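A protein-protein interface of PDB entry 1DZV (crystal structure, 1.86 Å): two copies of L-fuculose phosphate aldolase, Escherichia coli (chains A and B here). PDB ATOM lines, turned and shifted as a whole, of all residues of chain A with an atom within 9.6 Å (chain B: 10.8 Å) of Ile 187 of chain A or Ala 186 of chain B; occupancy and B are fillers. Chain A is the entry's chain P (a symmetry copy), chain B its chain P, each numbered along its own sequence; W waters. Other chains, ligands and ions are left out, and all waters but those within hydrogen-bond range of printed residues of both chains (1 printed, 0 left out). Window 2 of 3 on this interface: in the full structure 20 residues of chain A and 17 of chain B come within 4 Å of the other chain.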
ATOM      1  N   LEU A 180       3.093 -16.843   9.880  1.00  0.00           N
ATOM      2  CA  LEU A 180       3.385 -15.458   9.517  1.00  0.00           C
ATOM      3  C   LEU A 180       4.286 -15.387   8.273  1.00  0.00           C
ATOM      4  O   LEU A 180       4.096 -14.592   7.360  1.00  0.00           O
ATOM      5  CB  LEU A 180       4.074 -14.696  10.652  1.00  0.00           C
ATOM      6  CG  LEU A 180       3.209 -14.399  11.875  1.00  0.00           C
ATOM      7  CD1 LEU A 180       4.079 -13.847  12.995  1.00  0.00           C
ATOM      8  CD2 LEU A 180       2.091 -13.411  11.508  1.00  0.00           C
ATOM      9  N   TYR A 181       5.316 -16.210   8.237  1.00  0.00           N
ATOM     10  CA  TYR A 181       6.279 -16.306   7.168  1.00  0.00           C
ATOM     11  C   TYR A 181       5.649 -16.726   5.839  1.00  0.00           C
ATOM     12  O   TYR A 181       5.855 -16.049   4.824  1.00  0.00           O
ATOM     13  CB  TYR A 181       7.398 -17.284   7.588  1.00  0.00           C
ATOM     14  CG  TYR A 181       8.611 -17.125   6.677  1.00  0.00           C
ATOM     15  CD1 TYR A 181       8.996 -15.888   6.175  1.00  0.00           C
ATOM     16  CD2 TYR A 181       9.361 -18.244   6.324  1.00  0.00           C
ATOM     17  CE1 TYR A 181      10.086 -15.768   5.330  1.00  0.00           C
ATOM     18  CE2 TYR A 181      10.455 -18.134   5.491  1.00  0.00           C
ATOM     19  CZ  TYR A 181      10.813 -16.891   4.997  1.00  0.00           C
ATOM     20  OH  TYR A 181      11.899 -16.770   4.153  1.00  0.00           O
ATOM     21  N   LEU A 182       4.845 -17.790   5.839  1.00  0.00           N
ATOM     22  CA  LEU A 182       4.216 -18.230   4.605  1.00  0.00           C
ATOM     23  C   LEU A 182       3.208 -17.213   4.063  1.00  0.00           C
ATOM     24  O   LEU A 182       3.097 -16.990   2.851  1.00  0.00           O
ATOM     25  CB  LEU A 182       3.496 -19.559   4.835  1.00  0.00           C
ATOM     26  CG  LEU A 182       4.400 -20.761   5.116  1.00  0.00           C
ATOM     27  CD1 LEU A 182       3.600 -21.850   5.807  1.00  0.00           C
ATOM     28  CD2 LEU A 182       5.020 -21.223   3.807  1.00  0.00           C
ATOM     29  N   THR A 183       2.426 -16.615   4.962  1.00  0.00           N
ATOM     30  CA  THR A 183       1.423 -15.633   4.587  1.00  0.00           C
ATOM     31  C   THR A 183       2.075 -14.411   3.948  1.00  0.00           C
ATOM     32  O   THR A 183       1.602 -13.989   2.892  1.00  0.00           O
ATOM     33  CB  THR A 183       0.602 -15.204   5.821  1.00  0.00           C
ATOM     34  OG1 THR A 183       0.012 -16.407   6.370  1.00  0.00           O
ATOM     35  CG2 THR A 183      -0.479 -14.211   5.458  1.00  0.00           C
ATOM     36  N   THR A 184       3.180 -13.918   4.493  1.00  0.00           N
ATOM     37  CA  THR A 184       3.869 -12.776   3.913  1.00  0.00           C
ATOM     38  C   THR A 184       4.720 -13.163   2.707  1.00  0.00           C
ATOM     39  O   THR A 184       4.790 -12.338   1.787  1.00  0.00           O
ATOM     40  CB  THR A 184       4.722 -12.035   4.952  1.00  0.00           C
ATOM     41  OG1 THR A 184       5.628 -12.930   5.615  1.00  0.00           O
ATOM     42  CG2 THR A 184       3.808 -11.439   6.022  1.00  0.00           C
ATOM     43  N   LEU A 185       5.300 -14.356   2.620  1.00  0.00           N
ATOM     44  CA  LEU A 185       6.070 -14.776   1.467  1.00  0.00           C
ATOM     45  C   LEU A 185       5.231 -14.863   0.190  1.00  0.00           C
ATOM     46  O   LEU A 185       5.774 -14.755  -0.899  1.00  0.00           O
ATOM     47  CB  LEU A 185       6.644 -16.193   1.634  1.00  0.00           C
ATOM     48  CG  LEU A 185       8.118 -16.378   1.906  1.00  0.00           C
ATOM     49  CD1 LEU A 185       8.500 -17.830   1.578  1.00  0.00           C
ATOM     50  CD2 LEU A 185       9.014 -15.409   1.140  1.00  0.00           C
ATOM     51  N   ALA A 186       3.937 -15.149   0.298  1.00  0.00           N
ATOM     52  CA  ALA A 186       3.031 -15.225  -0.824  1.00  0.00           C
ATOM     53  C   ALA A 186       2.825 -13.844  -1.457  1.00  0.00           C
ATOM     54  O   ALA A 186       2.470 -13.772  -2.628  1.00  0.00           O
ATOM     55  CB  ALA A 186       1.645 -15.728  -0.428  1.00  0.00           C
ATOM     56  N   ILE A 187       2.978 -12.805  -0.670  1.00  0.00           N
ATOM     57  CA  ILE A 187       2.814 -11.430  -1.093  1.00  0.00           C
ATOM     58  C   ILE A 187       4.143 -10.833  -1.548  1.00  0.00           C
ATOM     59  O   ILE A 187       4.159 -10.181  -2.581  1.00  0.00           O
ATOM     60  CB  ILE A 187       2.268 -10.574   0.064  1.00  0.00           C
ATOM     61  CG1 ILE A 187       0.929 -11.077   0.605  1.00  0.00           C
ATOM     62  CG2 ILE A 187       2.177  -9.099  -0.308  1.00  0.00           C
ATOM     63  CD1 ILE A 187      -0.019 -11.704  -0.365  1.00  0.00           C
ATOM     64  N   THR A 188       5.195 -10.958  -0.765  1.00  0.00           N
ATOM     65  CA  THR A 188       6.486 -10.372  -1.098  1.00  0.00           C
ATOM     66  C   THR A 188       7.659 -11.270  -0.705  1.00  0.00           C
ATOM     67  O   THR A 188       7.653 -11.892   0.362  1.00  0.00           O
ATOM     68  CB  THR A 188       6.680  -8.988  -0.443  1.00  0.00           C
ATOM     69  OG1 THR A 188       7.967  -8.493  -0.862  1.00  0.00           O
ATOM     70  CG2 THR A 188       6.711  -9.048   1.074  1.00  0.00           C
ATOM     71  N   ASP A 189       8.681 -11.331  -1.549  1.00  0.00           N
ATOM     72  CA  ASP A 189       9.880 -12.130  -1.314  1.00  0.00           C
ATOM     73  C   ASP A 189      11.088 -11.324  -1.794  1.00  0.00           C
ATOM     74  O   ASP A 189      11.128 -10.963  -2.980  1.00  0.00           O
ATOM     75  CB  ASP A 189       9.823 -13.463  -2.059  1.00  0.00           C
ATOM     76  CG  ASP A 189      10.960 -14.416  -1.760  1.00  0.00           C
ATOM     77  OD1 ASP A 189      12.018 -14.034  -1.215  1.00  0.00           O
ATOM     78  OD2 ASP A 189      10.805 -15.618  -2.063  1.00  0.00           O
ATOM     79  N   PRO A 190      11.986 -10.994  -0.875  1.00  0.00           N
ATOM     80  CA  PRO A 190      11.965 -11.460   0.489  1.00  0.00           C
ATOM     81  C   PRO A 190      11.129 -10.666   1.477  1.00  0.00           C
ATOM     82  O   PRO A 190      10.763  -9.525   1.232  1.00  0.00           O
ATOM     83  CB  PRO A 190      13.460 -11.400   0.864  1.00  0.00           C
ATOM     84  CG  PRO A 190      13.961 -10.188   0.147  1.00  0.00           C
ATOM     85  CD  PRO A 190      13.231 -10.225  -1.179  1.00  0.00           C
ATOM     86  N   VAL A 191      10.819 -11.275   2.617  1.00  0.00           N
ATOM     87  CA  VAL A 191      10.007 -10.637   3.658  1.00  0.00           C
ATOM     88  C   VAL A 191      10.855  -9.724   4.531  1.00  0.00           C
ATOM     89  O   VAL A 191      11.939 -10.102   4.954  1.00  0.00           O
ATOM     90  CB  VAL A 191       9.364 -11.703   4.577  1.00  0.00           C
ATOM     91  CG1 VAL A 191       8.609 -11.013   5.723  1.00  0.00           C
ATOM     92  CG2 VAL A 191       8.382 -12.596   3.822  1.00  0.00           C
ATOM     93  N   PRO A 192      10.353  -8.540   4.864  1.00  0.00           N
ATOM     94  CA  PRO A 192      11.078  -7.620   5.731  1.00  0.00           C
ATOM     95  C   PRO A 192      11.529  -8.304   6.998  1.00  0.00           C
ATOM     96  O   PRO A 192      10.739  -9.083   7.511  1.00  0.00           O
ATOM     97  CB  PRO A 192      10.045  -6.538   6.055  1.00  0.00           C
ATOM     98  CG  PRO A 192       9.209  -6.523   4.807  1.00  0.00           C
ATOM     99  CD  PRO A 192       9.075  -7.978   4.398  1.00  0.00           C
ATOM    100  N   HIS B  97      -3.308 -12.577  11.398  1.00  0.00           N
ATOM    101  CA  HIS B  97      -3.470 -11.762  10.186  1.00  0.00           C
ATOM    102  C   HIS B  97      -3.033 -10.322  10.399  1.00  0.00           C
ATOM    103  O   HIS B  97      -2.296  -9.743   9.600  1.00  0.00           O
ATOM    104  CB  HIS B  97      -4.914 -11.864   9.643  1.00  0.00           C
ATOM    105  CG  HIS B  97      -5.220 -13.296   9.302  1.00  0.00           C
ATOM    106  ND1 HIS B  97      -5.944 -14.139  10.100  1.00  0.00           N
ATOM    107  CD2 HIS B  97      -4.837 -14.019   8.202  1.00  0.00           C
ATOM    108  CE1 HIS B  97      -6.000 -15.329   9.511  1.00  0.00           C
ATOM    109  NE2 HIS B  97      -5.359 -15.283   8.348  1.00  0.00           N
ATOM    110  N   THR B  99      -0.869  -9.234  12.538  1.00  0.00           N
ATOM    111  CA  THR B  99       0.603  -9.272  12.656  1.00  0.00           C
ATOM    112  C   THR B  99       1.258  -9.472  11.302  1.00  0.00           C
ATOM    113  O   THR B  99       2.287  -8.814  11.025  1.00  0.00           O
ATOM    114  CB  THR B  99       1.014 -10.362  13.665  1.00  0.00           C
ATOM    115  OG1 THR B  99       0.339 -10.122  14.919  1.00  0.00           O
ATOM    116  CG2 THR B  99       2.526 -10.319  13.886  1.00  0.00           C
ATOM    117  N   ALA B 100       0.678 -10.263  10.396  1.00  0.00           N
ATOM    118  CA  ALA B 100       1.281 -10.448   9.062  1.00  0.00           C
ATOM    119  C   ALA B 100       1.223  -9.125   8.300  1.00  0.00           C
ATOM    120  O   ALA B 100       2.201  -8.715   7.654  1.00  0.00           O
ATOM    121  CB  ALA B 100       0.635 -11.535   8.222  1.00  0.00           C
ATOM    122  N   VAL B 101       0.103  -8.407   8.459  1.00  0.00           N
ATOM    123  CA  VAL B 101       0.032  -7.087   7.805  1.00  0.00           C
ATOM    124  C   VAL B 101       1.079  -6.164   8.425  1.00  0.00           C
ATOM    125  O   VAL B 101       1.713  -5.413   7.667  1.00  0.00           O
ATOM    126  CB  VAL B 101      -1.334  -6.428   7.856  1.00  0.00           C
ATOM    127  CG1 VAL B 101      -1.314  -5.040   7.201  1.00  0.00           C
ATOM    128  CG2 VAL B 101      -2.342  -7.328   7.125  1.00  0.00           C
ATOM    129  N   SER B 102       1.294  -6.260   9.745  1.00  0.00           N
ATOM    130  CA  SER B 102       2.289  -5.402  10.381  1.00  0.00           C
ATOM    131  C   SER B 102       3.710  -5.702   9.922  1.00  0.00           C
ATOM    132  O   SER B 102       4.556  -4.789   9.964  1.00  0.00           O
ATOM    133  CB  SER B 102       2.214  -5.502  11.904  1.00  0.00           C
ATOM    134  OG  SER B 102       3.005  -6.581  12.365  1.00  0.00           O
ATOM    135  N   ILE B 103       3.968  -6.929   9.498  1.00  0.00           N
ATOM    136  CA  ILE B 103       5.280  -7.284   8.961  1.00  0.00           C
ATOM    137  C   ILE B 103       5.519  -6.623   7.621  1.00  0.00           C
ATOM    138  O   ILE B 103       6.623  -6.158   7.296  1.00  0.00           O
ATOM    139  CB  ILE B 103       5.389  -8.818   8.911  1.00  0.00           C
ATOM    140  CG1 ILE B 103       5.551  -9.327  10.343  1.00  0.00           C
ATOM    141  CG2 ILE B 103       6.563  -9.264   8.083  1.00  0.00           C
ATOM    142  CD1 ILE B 103       5.364 -10.819  10.512  1.00  0.00           C
ATOM    143  N   LEU B 104       4.508  -6.474   6.789  1.00  0.00           N
ATOM    144  CA  LEU B 104       4.601  -5.818   5.496  1.00  0.00           C
ATOM    145  C   LEU B 104       4.704  -4.314   5.701  1.00  0.00           C
ATOM    146  O   LEU B 104       5.053  -3.566   4.788  1.00  0.00           O
ATOM    147  CB  LEU B 104       3.401  -6.179   4.607  1.00  0.00           C
ATOM    148  CG  LEU B 104       3.190  -7.674   4.321  1.00  0.00           C
ATOM    149  CD1 LEU B 104       1.911  -7.950   3.534  1.00  0.00           C
ATOM    150  CD2 LEU B 104       4.385  -8.254   3.585  1.00  0.00           C
ATOM    151  N   ASN B 105       4.339  -3.827   6.891  1.00  0.00           N
ATOM    152  CA  ASN B 105       4.390  -2.428   7.223  1.00  0.00           C
ATOM    153  C   ASN B 105       3.392  -1.656   6.367  1.00  0.00           C
ATOM    154  O   ASN B 105       3.657  -0.563   5.881  1.00  0.00           O
ATOM    155  CB  ASN B 105       5.802  -1.820   7.068  1.00  0.00           C
ATOM    156  CG  ASN B 105       5.912  -0.490   7.779  1.00  0.00           C
ATOM    157  OD1 ASN B 105       5.154  -0.225   8.721  1.00  0.00           O
ATOM    158  ND2 ASN B 105       6.829   0.372   7.349  1.00  0.00           N
ATOM    159  N   ARG B 106       2.196  -2.217   6.203  1.00  0.00           N
ATOM    160  CA  ARG B 106       1.161  -1.553   5.427  1.00  0.00           C
ATOM    161  C   ARG B 106       0.017  -1.137   6.332  1.00  0.00           C
ATOM    162  O   ARG B 106      -0.267  -1.875   7.284  1.00  0.00           O
ATOM    163  CB  ARG B 106       0.568  -2.550   4.411  1.00  0.00           C
ATOM    164  CG  ARG B 106       1.545  -2.928   3.312  1.00  0.00           C
ATOM    165  CD  ARG B 106       0.745  -3.379   2.097  1.00  0.00           C
ATOM    166  NE  ARG B 106       1.613  -3.897   1.055  1.00  0.00           N
ATOM    167  CZ  ARG B 106       1.321  -3.877  -0.244  1.00  0.00           C
ATOM    168  NH1 ARG B 106       0.168  -3.351  -0.641  1.00  0.00           N
ATOM    169  NH2 ARG B 106       2.177  -4.375  -1.137  1.00  0.00           N
ATOM    170  N   ILE B 111     -11.071  -1.504   2.205  1.00  0.00           N
ATOM    171  CA  ILE B 111     -11.484  -2.606   1.356  1.00  0.00           C
ATOM    172  C   ILE B 111     -12.870  -3.135   1.724  1.00  0.00           C
ATOM    173  O   ILE B 111     -13.465  -3.938   1.009  1.00  0.00           O
ATOM    174  CB  ILE B 111     -10.473  -3.760   1.464  1.00  0.00           C
ATOM    175  CG1 ILE B 111     -10.345  -4.199   2.926  1.00  0.00           C
ATOM    176  CG2 ILE B 111      -9.137  -3.279   0.902  1.00  0.00           C
ATOM    177  CD1 ILE B 111      -9.609  -5.506   3.112  1.00  0.00           C
ATOM    178  N   ALA B 178      -7.930  -7.582   8.306  1.00  0.00           N
ATOM    179  CA  ALA B 178      -6.562  -7.994   7.974  1.00  0.00           C
ATOM    180  C   ALA B 178      -6.518  -9.254   7.100  1.00  0.00           C
ATOM    181  O   ALA B 178      -5.812  -9.329   6.088  1.00  0.00           O
ATOM    182  CB  ALA B 178      -5.766  -8.223   9.284  1.00  0.00           C
ATOM    183  N   GLN B 179      -7.330 -10.245   7.479  1.00  0.00           N
ATOM    184  CA  GLN B 179      -7.487 -11.476   6.746  1.00  0.00           C
ATOM    185  C   GLN B 179      -8.075 -11.197   5.366  1.00  0.00           C
ATOM    186  O   GLN B 179      -7.571 -11.734   4.394  1.00  0.00           O
ATOM    187  CB  GLN B 179      -8.392 -12.479   7.466  1.00  0.00           C
ATOM    188  CG  GLN B 179      -8.227 -13.861   6.822  1.00  0.00           C
ATOM    189  CD  GLN B 179      -9.098 -14.923   7.470  1.00  0.00           C
ATOM    190  OE1 GLN B 179      -9.655 -14.673   8.536  1.00  0.00           O
ATOM    191  NE2 GLN B 179      -9.213 -16.077   6.810  1.00  0.00           N
ATOM    192  N   LEU B 180      -9.074 -10.320   5.268  1.00  0.00           N
ATOM    193  CA  LEU B 180      -9.613  -9.948   3.961  1.00  0.00           C
ATOM    194  C   LEU B 180      -8.527  -9.330   3.067  1.00  0.00           C
ATOM    195  O   LEU B 180      -8.402  -9.614   1.881  1.00  0.00           O
ATOM    196  CB  LEU B 180     -10.767  -8.949   4.075  1.00  0.00           C
ATOM    197  CG  LEU B 180     -12.063  -9.493   4.672  1.00  0.00           C
ATOM    198  CD1 LEU B 180     -13.029  -8.346   4.928  1.00  0.00           C
ATOM    199  CD2 LEU B 180     -12.684 -10.537   3.732  1.00  0.00           C
ATOM    200  N   TYR B 181      -7.734  -8.437   3.626  1.00  0.00           N
ATOM    201  CA  TYR B 181      -6.655  -7.741   2.968  1.00  0.00           C
ATOM    202  C   TYR B 181      -5.561  -8.684   2.466  1.00  0.00           C
ATOM    203  O   TYR B 181      -5.191  -8.619   1.287  1.00  0.00           O
ATOM    204  CB  TYR B 181      -6.078  -6.683   3.935  1.00  0.00           C
ATOM    205  CG  TYR B 181      -5.218  -5.681   3.172  1.00  0.00           C
ATOM    206  CD1 TYR B 181      -5.538  -5.267   1.886  1.00  0.00           C
ATOM    207  CD2 TYR B 181      -4.071  -5.162   3.767  1.00  0.00           C
ATOM    208  CE1 TYR B 181      -4.731  -4.375   1.200  1.00  0.00           C
ATOM    209  CE2 TYR B 181      -3.265  -4.264   3.098  1.00  0.00           C
ATOM    210  CZ  TYR B 181      -3.602  -3.873   1.813  1.00  0.00           C
ATOM    211  OH  TYR B 181      -2.797  -2.985   1.128  1.00  0.00           O
ATOM    212  N   LEU B 182      -5.080  -9.591   3.317  1.00  0.00           N
ATOM    213  CA  LEU B 182      -4.043 -10.515   2.892  1.00  0.00           C
ATOM    214  C   LEU B 182      -4.527 -11.486   1.812  1.00  0.00           C
ATOM    215  O   LEU B 182      -3.801 -11.825   0.868  1.00  0.00           O
ATOM    216  CB  LEU B 182      -3.543 -11.323   4.090  1.00  0.00           C
ATOM    217  CG  LEU B 182      -2.774 -10.530   5.148  1.00  0.00           C
ATOM    218  CD1 LEU B 182      -2.786 -11.290   6.462  1.00  0.00           C
ATOM    219  CD2 LEU B 182      -1.370 -10.261   4.633  1.00  0.00           C
ATOM    220  N   THR B 183      -5.754 -11.983   1.967  1.00  0.00           N
ATOM    221  CA  THR B 183      -6.338 -12.919   1.022  1.00  0.00           C
ATOM    222  C   THR B 183      -6.484 -12.276  -0.354  1.00  0.00           C
ATOM    223  O   THR B 183      -6.086 -12.909  -1.333  1.00  0.00           O
ATOM    224  CB  THR B 183      -7.716 -13.402   1.524  1.00  0.00           C
ATOM    225  OG1 THR B 183      -7.500 -14.001   2.823  1.00  0.00           O
ATOM    226  CG2 THR B 183      -8.334 -14.409   0.580  1.00  0.00           C
ATOM    227  N   THR B 184      -6.935 -11.030  -0.433  1.00  0.00           N
ATOM    228  CA  THR B 184      -7.065 -10.349  -1.711  1.00  0.00           C
ATOM    229  C   THR B 184      -5.728  -9.825  -2.228  1.00  0.00           C
ATOM    230  O   THR B 184      -5.555  -9.854  -3.454  1.00  0.00           O
ATOM    231  CB  THR B 184      -8.095  -9.212  -1.651  1.00  0.00           C
ATOM    232  OG1 THR B 184      -7.801  -8.300  -0.582  1.00  0.00           O
ATOM    233  CG2 THR B 184      -9.479  -9.801  -1.378  1.00  0.00           C
ATOM    234  N   LEU B 185      -4.770  -9.423  -1.398  1.00  0.00           N
ATOM    235  CA  LEU B 185      -3.471  -8.971  -1.852  1.00  0.00           C
ATOM    236  C   LEU B 185      -2.676 -10.066  -2.566  1.00  0.00           C
ATOM    237  O   LEU B 185      -1.812  -9.758  -3.373  1.00  0.00           O
ATOM    238  CB  LEU B 185      -2.561  -8.548  -0.687  1.00  0.00           C
ATOM    239  CG  LEU B 185      -2.293  -7.082  -0.439  1.00  0.00           C
ATOM    240  CD1 LEU B 185      -1.041  -6.955   0.444  1.00  0.00           C
ATOM    241  CD2 LEU B 185      -2.127  -6.261  -1.714  1.00  0.00           C
ATOM    242  N   ALA B 186      -2.884 -11.332  -2.218  1.00  0.00           N
ATOM    243  CA  ALA B 186      -2.225 -12.458  -2.838  1.00  0.00           C
ATOM    244  C   ALA B 186      -2.682 -12.628  -4.292  1.00  0.00           C
ATOM    245  O   ALA B 186      -1.949 -13.211  -5.082  1.00  0.00           O
ATOM    246  CB  ALA B 186      -2.530 -13.778  -2.135  1.00  0.00           C
ATOM    247  N   ILE B 187      -3.882 -12.188  -4.590  1.00  0.00           N
ATOM    248  CA  ILE B 187      -4.478 -12.273  -5.906  1.00  0.00           C
ATOM    249  C   ILE B 187      -4.204 -11.010  -6.717  1.00  0.00           C
ATOM    250  O   ILE B 187      -3.851 -11.135  -7.879  1.00  0.00           O
ATOM    251  CB  ILE B 187      -6.003 -12.455  -5.793  1.00  0.00           C
ATOM    252  CG1 ILE B 187      -6.404 -13.699  -4.999  1.00  0.00           C
ATOM    253  CG2 ILE B 187      -6.684 -12.447  -7.156  1.00  0.00           C
ATOM    254  CD1 ILE B 187      -5.519 -14.899  -5.097  1.00  0.00           C
ATOM    255  N   THR B 188      -4.450  -9.838  -6.167  1.00  0.00           N
ATOM    256  CA  THR B 188      -4.267  -8.587  -6.889  1.00  0.00           C
ATOM    257  C   THR B 188      -3.709  -7.473  -6.003  1.00  0.00           C
ATOM    258  O   THR B 188      -4.103  -7.326  -4.842  1.00  0.00           O
ATOM    259  CB  THR B 188      -5.578  -8.094  -7.536  1.00  0.00           C
ATOM    260  OG1 THR B 188      -5.275  -6.876  -8.244  1.00  0.00           O
ATOM    261  CG2 THR B 188      -6.651  -7.749  -6.519  1.00  0.00           C
ATOM    262  N   ASP B 189      -2.803  -6.668  -6.546  1.00  0.00           N
ATOM    263  CA  ASP B 189      -2.185  -5.549  -5.839  1.00  0.00           C
ATOM    264  C   ASP B 189      -2.053  -4.384  -6.820  1.00  0.00           C
ATOM    265  O   ASP B 189      -1.397  -4.553  -7.860  1.00  0.00           O
ATOM    266  CB  ASP B 189      -0.806  -5.922  -5.294  1.00  0.00           C
ATOM    267  CG  ASP B 189      -0.153  -4.869  -4.426  1.00  0.00           C
ATOM    268  OD1 ASP B 189      -0.543  -3.682  -4.417  1.00  0.00           O
ATOM    269  OD2 ASP B 189       0.794  -5.227  -3.693  1.00  0.00           O
ATOM    270  N   PRO B 190      -2.724  -3.279  -6.524  1.00  0.00           N
ATOM    271  CA  PRO B 190      -3.439  -3.065  -5.291  1.00  0.00           C
ATOM    272  C   PRO B 190      -4.869  -3.571  -5.226  1.00  0.00           C
ATOM    273  O   PRO B 190      -5.498  -3.843  -6.239  1.00  0.00           O
ATOM    274  CB  PRO B 190      -3.396  -1.528  -5.166  1.00  0.00           C
ATOM    275  CG  PRO B 190      -3.514  -1.050  -6.577  1.00  0.00           C
ATOM    276  CD  PRO B 190      -2.689  -2.044  -7.365  1.00  0.00           C
ATOM    277  N   VAL B 191      -5.398  -3.704  -4.014  1.00  0.00           N
ATOM    278  CA  VAL B 191      -6.763  -4.194  -3.796  1.00  0.00           C
ATOM    279  C   VAL B 191      -7.781  -3.078  -3.973  1.00  0.00           C
ATOM    280  O   VAL B 191      -7.595  -1.981  -3.463  1.00  0.00           O
ATOM    281  CB  VAL B 191      -6.920  -4.750  -2.360  1.00  0.00           C
ATOM    282  CG1 VAL B 191      -8.380  -5.157  -2.119  1.00  0.00           C
ATOM    283  CG2 VAL B 191      -6.033  -5.969  -2.116  1.00  0.00           C
ATOM    284  N   PRO B 192      -8.895  -3.352  -4.643  1.00  0.00           N
ATOM    285  CA  PRO B 192      -9.942  -2.355  -4.825  1.00  0.00           C
ATOM    286  C   PRO B 192     -10.336  -1.731  -3.509  1.00  0.00           C
ATOM    287  O   PRO B 192     -10.410  -2.481  -2.547  1.00  0.00           O
ATOM    288  CB  PRO B 192     -11.112  -3.160  -5.396  1.00  0.00           C
ATOM    289  CG  PRO B 192     -10.402  -4.234  -6.171  1.00  0.00           C
ATOM    290  CD  PRO B 192      -9.212  -4.624  -5.313  1.00  0.00           C
HETATM  291  O   HOH W   1       1.305 -12.792  -5.162  1.00  0.00           O
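Water W1 lies within hydrogen-bond range of the backbone carbonyl oxygen (O) of Ala 186 of chain A (3.0 Å) and the backbone carbonyl oxygen (O) of Ala 186 of chain B (3.3 Å).
Thr 183 of chain A touches Leu 182 of chain B, but with the chains exchanged Leu 182 of chain A does not touch Thr 183 of chain B (10.2 Å). Ile 187 of chain A touches Leu 182 of chain B, but with the chains exchanged Leu 182 of chain A does not touch Ile 187 of chain B (11.3 Å). Ile 187 of chain A touches Leu 185 of chain B, but with the chains exchanged Leu 185 of chain A does not touch Ile 187 of chain B (10.6 Å). Ile 187 of chain A touches Ala 186 of chain B, but with the chains exchanged Ala 186 of chain A does not touch Ile 187 of chain B (6.8 Å). Of the 10 pairs that touch across the chains among the printed residues, none has its exchanged pair printed and touching as well.
OG1 of Thr 184 of chain A is in hydrogen-bond range of O of Leu 180 of chain A (2.9 Å). OG of Ser 102 of chain B is in hydrogen-bond range of O of Thr 99 of chain B. The side-chain hydroxyl (OG1) of Thr 184 of chain A sits at hydrogen-bond distance from the backbone carbonyl oxygen (O) of Tyr 181 of chain A (3.2 Å).
Printed residues of chain A that touch a printed residue of chain B: Leu 180, Thr 183, Thr 184, Ile 187, Thr 188, Val 191 and Pro 192. Along chain A the printed residues that touch a printed residue of chain B span positions 180 to 192. Of the 25 printed residues of chain B, 7 touch a printed residue of chain A. Printed residues of chain B that touch a printed residue of chain A: Thr 99, Ala 100, Ile 103, Leu 104, Leu 182, Leu 185 and Ala 186. Among the printed residues, 10 pairs touch across the chains. Among the printed residues, no Asp or Glu carboxylate lies within 4 Å of a Lys or Arg side-chain nitrogen of the other chain.
Among the printed residues, merely in contact across the chains: Ile 187 of chain A with Ala 186 of chain B (3.4 Å), Thr 188 of chain A with Leu 104 of chain B (3.5 Å), Thr 184 of chain A with Ala 100 of chain B (3.6 Å), Val 191 of chain A with Ile 103 of chain B (3.6 Å), Pro 192 of chain A with Ile 103 of chain B (3.6 Å), Leu 180 of chain A with Ala 100 of chain B (3.6 Å), Ile 187 of chain A with Leu 185 of chain B (3.8 Å), Thr 183 of chain A with Leu 182 of chain B (3.9 Å), Leu 180 of chain A with Thr 99 of chain B (3.9 Å) and Ile 187 of chain A with Leu 182 of chain B (3.98 Å).
Printed residues of chain B within 4 Å of Thr 184 of chain A: Ala 100. Of the printed residues of chain B, Ile 187 of chain A touches Leu 182 (3.98 Å), Leu 185 (3.8 Å) and Ala 186 (3.4 Å). Thr 188 of chain A touches just one residue of chain B: Leu 104 (3.5 Å). Of the printed residues of chain A, Thr 99 of chain B touches Leu 180. Ile 111 of chain B touches none of the printed residues of chain A. Printed residues of chain A within 4 Å of Leu 182 of chain B: Thr 183 and Ile 187. Leu 185 of chain B touches just one residue of chain A: Ile 187 (3.8 Å). Ala 186 of chain B touches one residue of chain A. No residue of chain A comes within 4 Å of Ile 187 of chain B. The nearest residue of chain A that does not touch Ala 186 of chain B is Ala 186 of chain A (4.9 Å). The nearest printed residue of chain B that does not touch Val 191 of chain A is Leu 104 of chain B (5.5 Å).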
